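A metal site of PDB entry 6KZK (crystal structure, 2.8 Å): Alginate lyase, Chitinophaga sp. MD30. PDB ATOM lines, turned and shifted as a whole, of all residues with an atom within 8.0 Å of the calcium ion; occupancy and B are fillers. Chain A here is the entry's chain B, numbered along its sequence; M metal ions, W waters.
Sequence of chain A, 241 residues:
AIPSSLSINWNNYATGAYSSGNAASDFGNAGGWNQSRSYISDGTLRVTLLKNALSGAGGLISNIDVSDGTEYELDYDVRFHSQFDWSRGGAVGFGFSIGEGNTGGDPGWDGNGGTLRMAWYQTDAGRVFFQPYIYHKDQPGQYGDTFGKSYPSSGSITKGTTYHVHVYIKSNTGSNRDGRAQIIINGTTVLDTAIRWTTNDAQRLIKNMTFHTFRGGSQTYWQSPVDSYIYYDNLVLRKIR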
ATOM      1  N   ILE A   8      25.125  12.090  -4.358  1.00  0.00           N
ATOM      2  CA  ILE A   8      26.373  12.500  -3.731  1.00  0.00           C
ATOM      3  C   ILE A   8      26.409  11.893  -2.337  1.00  0.00           C
ATOM      4  O   ILE A   8      25.454  12.047  -1.569  1.00  0.00           O
ATOM      5  CB  ILE A   8      26.525  14.024  -3.676  1.00  0.00           C
ATOM      6  CG1 ILE A   8      26.319  14.635  -5.056  1.00  0.00           C
ATOM      7  CG2 ILE A   8      27.897  14.362  -3.168  1.00  0.00           C
ATOM      8  CD1 ILE A   8      26.234  16.149  -5.049  1.00  0.00           C
ATOM      9  N   ASN A   9      27.491  11.188  -2.034  1.00  0.00           N
ATOM     10  CA  ASN A   9      27.662  10.606  -0.722  1.00  0.00           C
ATOM     11  C   ASN A   9      29.015  10.957  -0.090  1.00  0.00           C
ATOM     12  O   ASN A   9      29.282  10.537   1.045  1.00  0.00           O
ATOM     13  CB  ASN A   9      27.473   9.072  -0.788  1.00  0.00           C
ATOM     14  CG  ASN A   9      28.387   8.416  -1.789  1.00  0.00           C
ATOM     15  OD1 ASN A   9      29.582   8.674  -1.831  1.00  0.00           O
ATOM     16  ND2 ASN A   9      27.817   7.560  -2.618  1.00  0.00           N
ATOM     17  N   TRP A  10      29.859  11.717  -0.791  1.00  0.00           N
ATOM     18  CA  TRP A  10      31.141  12.209  -0.273  1.00  0.00           C
ATOM     19  C   TRP A  10      32.060  11.085   0.221  1.00  0.00           C
ATOM     20  O   TRP A  10      32.957  11.322   1.038  1.00  0.00           O
ATOM     21  CB  TRP A  10      30.915  13.253   0.827  1.00  0.00           C
ATOM     22  CG  TRP A  10      30.173  14.475   0.319  1.00  0.00           C
ATOM     23  CD1 TRP A  10      30.702  15.562  -0.314  1.00  0.00           C
ATOM     24  CD2 TRP A  10      28.761  14.724   0.405  1.00  0.00           C
ATOM     25  NE1 TRP A  10      29.716  16.469  -0.630  1.00  0.00           N
ATOM     26  CE2 TRP A  10      28.520  15.971  -0.200  1.00  0.00           C
ATOM     27  CE3 TRP A  10      27.687  14.005   0.936  1.00  0.00           C
ATOM     28  CZ2 TRP A  10      27.245  16.507  -0.285  1.00  0.00           C
ATOM     29  CZ3 TRP A  10      26.416  14.548   0.847  1.00  0.00           C
ATOM     30  CH2 TRP A  10      26.215  15.784   0.241  1.00  0.00           C
ATOM     31  N   ASN A  11      31.885   9.854  -0.246  1.00  0.00           N
ATOM     32  CA  ASN A  11      32.718   8.758   0.234  1.00  0.00           C
ATOM     33  C   ASN A  11      34.108   8.734  -0.388  1.00  0.00           C
ATOM     34  O   ASN A  11      34.900   7.849  -0.053  1.00  0.00           O
ATOM     35  CB  ASN A  11      32.041   7.420  -0.020  1.00  0.00           C
ATOM     36  CG  ASN A  11      30.836   7.224   0.844  1.00  0.00           C
ATOM     37  OD1 ASN A  11      30.506   8.069   1.667  1.00  0.00           O
ATOM     38  ND2 ASN A  11      30.157   6.113   0.649  1.00  0.00           N
ATOM     39  N   ASN A  12      34.434   9.676  -1.265  1.00  0.00           N
ATOM     40  CA  ASN A  12      35.639   9.601  -2.072  1.00  0.00           C
ATOM     41  C   ASN A  12      36.692  10.615  -1.642  1.00  0.00           C
ATOM     42  O   ASN A  12      37.596  10.928  -2.418  1.00  0.00           O
ATOM     43  CB  ASN A  12      35.277   9.804  -3.545  1.00  0.00           C
ATOM     44  CG  ASN A  12      33.952   9.135  -3.901  1.00  0.00           C
ATOM     45  OD1 ASN A  12      32.886   9.776  -3.860  1.00  0.00           O
ATOM     46  ND2 ASN A  12      34.008   7.850  -4.261  1.00  0.00           N
ATOM     47  N   ILE A  40      35.410  17.766   4.612  1.00  0.00           N
ATOM     48  CA  ILE A  40      34.984  16.375   4.588  1.00  0.00           C
ATOM     49  C   ILE A  40      35.363  15.786   5.938  1.00  0.00           C
ATOM     50  O   ILE A  40      36.529  15.879   6.351  1.00  0.00           O
ATOM     51  CB  ILE A  40      35.602  15.592   3.429  1.00  0.00           C
ATOM     52  CG1 ILE A  40      35.125  16.172   2.100  1.00  0.00           C
ATOM     53  CG2 ILE A  40      35.178  14.119   3.507  1.00  0.00           C
ATOM     54  CD1 ILE A  40      33.632  16.021   1.890  1.00  0.00           C
ATOM     55  N   SER A  41      34.386  15.228   6.641  1.00  0.00           N
ATOM     56  CA  SER A  41      34.583  14.654   7.967  1.00  0.00           C
ATOM     57  C   SER A  41      34.043  13.235   7.919  1.00  0.00           C
ATOM     58  O   SER A  41      32.832  13.017   7.988  1.00  0.00           O
ATOM     59  CB  SER A  41      33.888  15.486   9.031  1.00  0.00           C
ATOM     60  OG  SER A  41      33.935  14.826  10.291  1.00  0.00           O
ATOM     61  N   ASP A  42      34.950  12.268   7.785  1.00  0.00           N
ATOM     62  CA  ASP A  42      34.595  10.858   7.840  1.00  0.00           C
ATOM     63  C   ASP A  42      33.460  10.560   6.854  1.00  0.00           C
ATOM     64  O   ASP A  42      32.353  10.152   7.218  1.00  0.00           O
ATOM     65  CB  ASP A  42      34.213  10.458   9.269  1.00  0.00           C
ATOM     66  CG  ASP A  42      33.988   8.970   9.404  1.00  0.00           C
ATOM     67  OD1 ASP A  42      34.713   8.187   8.770  1.00  0.00           O
ATOM     68  OD2 ASP A  42      33.059   8.602  10.156  1.00  0.00           O
ATOM     69  N   GLY A  43      33.748  10.816   5.589  1.00  0.00           N
ATOM     70  CA  GLY A  43      32.775  10.577   4.555  1.00  0.00           C
ATOM     71  C   GLY A  43      31.517  11.408   4.651  1.00  0.00           C
ATOM     72  O   GLY A  43      30.476  11.005   4.123  1.00  0.00           O
ATOM     73  N   THR A  44      31.563  12.566   5.318  1.00  0.00           N
ATOM     74  CA  THR A  44      30.425  13.462   5.357  1.00  0.00           C
ATOM     75  C   THR A  44      30.878  14.892   5.055  1.00  0.00           C
ATOM     76  O   THR A  44      32.032  15.248   5.289  1.00  0.00           O
ATOM     77  CB  THR A  44      29.689  13.392   6.720  1.00  0.00           C
ATOM     78  OG1 THR A  44      30.556  13.839   7.749  1.00  0.00           O
ATOM     79  CG2 THR A  44      29.247  11.962   7.032  1.00  0.00           C
ATOM     80  N   LEU A  45      29.968  15.695   4.507  1.00  0.00           N
ATOM     81  CA  LEU A  45      30.255  17.091   4.205  1.00  0.00           C
ATOM     82  C   LEU A  45      29.777  17.946   5.359  1.00  0.00           C
ATOM     83  O   LEU A  45      28.564  18.048   5.608  1.00  0.00           O
ATOM     84  CB  LEU A  45      29.624  17.556   2.908  1.00  0.00           C
ATOM     85  CG  LEU A  45      29.502  19.069   2.737  1.00  0.00           C
ATOM     86  CD1 LEU A  45      30.844  19.801   2.858  1.00  0.00           C
ATOM     87  CD2 LEU A  45      28.851  19.355   1.392  1.00  0.00           C
ATOM     88  N   ASP A  77      20.579  13.183   4.379  1.00  0.00           N
ATOM     89  CA  ASP A  77      20.723  13.013   5.825  1.00  0.00           C
ATOM     90  C   ASP A  77      21.432  14.232   6.417  1.00  0.00           C
ATOM     91  O   ASP A  77      22.406  14.723   5.832  1.00  0.00           O
ATOM     92  CB  ASP A  77      21.489  11.725   6.134  1.00  0.00           C
ATOM     93  CG  ASP A  77      20.753  10.461   5.652  1.00  0.00           C
ATOM     94  OD1 ASP A  77      19.650  10.187   6.184  1.00  0.00           O
ATOM     95  OD2 ASP A  77      21.269   9.737   4.754  1.00  0.00           O
ATOM     96  N   TYR A 232      26.200  16.777   6.730  1.00  0.00           N
ATOM     97  CA  TYR A 232      25.294  16.334   5.671  1.00  0.00           C
ATOM     98  C   TYR A 232      25.777  15.039   5.014  1.00  0.00           C
ATOM     99  O   TYR A 232      26.984  14.754   4.971  1.00  0.00           O
ATOM    100  CB  TYR A 232      25.149  17.390   4.578  1.00  0.00           C
ATOM    101  CG  TYR A 232      24.484  18.658   5.025  1.00  0.00           C
ATOM    102  CD1 TYR A 232      23.108  18.735   5.108  1.00  0.00           C
ATOM    103  CD2 TYR A 232      25.237  19.782   5.328  1.00  0.00           C
ATOM    104  CE1 TYR A 232      22.499  19.879   5.499  1.00  0.00           C
ATOM    105  CE2 TYR A 232      24.639  20.931   5.738  1.00  0.00           C
ATOM    106  CZ  TYR A 232      23.269  20.975   5.815  1.00  0.00           C
ATOM    107  OH  TYR A 232      22.685  22.146   6.210  1.00  0.00           O
ATOM    108  N   ASP A 233      24.835  14.280   4.483  1.00  0.00           N
ATOM    109  CA  ASP A 233      25.215  13.043   3.800  1.00  0.00           C
ATOM    110  C   ASP A 233      24.108  12.551   2.871  1.00  0.00           C
ATOM    111  O   ASP A 233      22.918  12.743   3.135  1.00  0.00           O
ATOM    112  CB  ASP A 233      25.562  11.941   4.804  1.00  0.00           C
ATOM    113  CG  ASP A 233      26.565  10.969   4.240  1.00  0.00           C
ATOM    114  OD1 ASP A 233      26.848  11.074   3.025  1.00  0.00           O
ATOM    115  OD2 ASP A 233      27.063  10.102   5.007  1.00  0.00           O
ATOM    116  N   ASN A 234      24.535  11.899   1.797  1.00  0.00           N
ATOM    117  CA  ASN A 234      23.642  11.117   0.947  1.00  0.00           C
ATOM    118  C   ASN A 234      22.543  11.975   0.331  1.00  0.00           C
ATOM    119  O   ASN A 234      21.355  11.615   0.347  1.00  0.00           O
ATOM    120  CB  ASN A 234      23.079   9.909   1.711  1.00  0.00           C
ATOM    121  CG  ASN A 234      24.178   9.037   2.369  1.00  0.00           C
ATOM    122  OD1 ASN A 234      25.300   8.918   1.867  1.00  0.00           O
ATOM    123  ND2 ASN A 234      23.841   8.415   3.499  1.00  0.00           N
ATOM    124  N   LEU A 235      22.932  13.115  -0.228  1.00  0.00           N
ATOM    125  CA  LEU A 235      22.022  13.870  -1.073  1.00  0.00           C
ATOM    126  C   LEU A 235      21.715  13.055  -2.314  1.00  0.00           C
ATOM    127  O   LEU A 235      22.630  12.471  -2.917  1.00  0.00           O
ATOM    128  CB  LEU A 235      22.610  15.233  -1.476  1.00  0.00           C
ATOM    129  CG  LEU A 235      21.808  15.857  -2.647  1.00  0.00           C
ATOM    130  CD1 LEU A 235      20.492  16.395  -2.114  1.00  0.00           C
ATOM    131  CD2 LEU A 235      22.560  16.932  -3.380  1.00  0.00           C
HETATM  132 CA    CA M   1      29.059   9.396   3.206  1.00  0.00          CA
HETATM  133  O   HOH W   1      30.213   7.469   4.672  1.00  0.00           O
HETATM  134  O   HOH W   2      27.196   7.483   2.416  1.00  0.00           O
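Of the 16 residues printed, 4 come within 4 Å of the calcium ion.
The nearest printed residue that does not touch the calcium ion is Asn 234 (4.02 Å).
The calcium ion is bound by O of Gly 43 (2.3 Å), O of Asn 9 (2.5 Å), OD1 of Asn 11 (2.5 Å), water W1 (2.7 Å), OD2 of Asp 233 (2.8 Å), OD1 of Asp 233 (2.8 Å) and water W2 (2.8 Å).
O of Asp 233 is in hydrogen-bond range of N of Asp 77 (2.7 Å).
The side-chain carboxylate (OD1) of Asp 233 lies close to the side-chain amide oxygen (OD1) of Asn 234 (2.9 Å).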
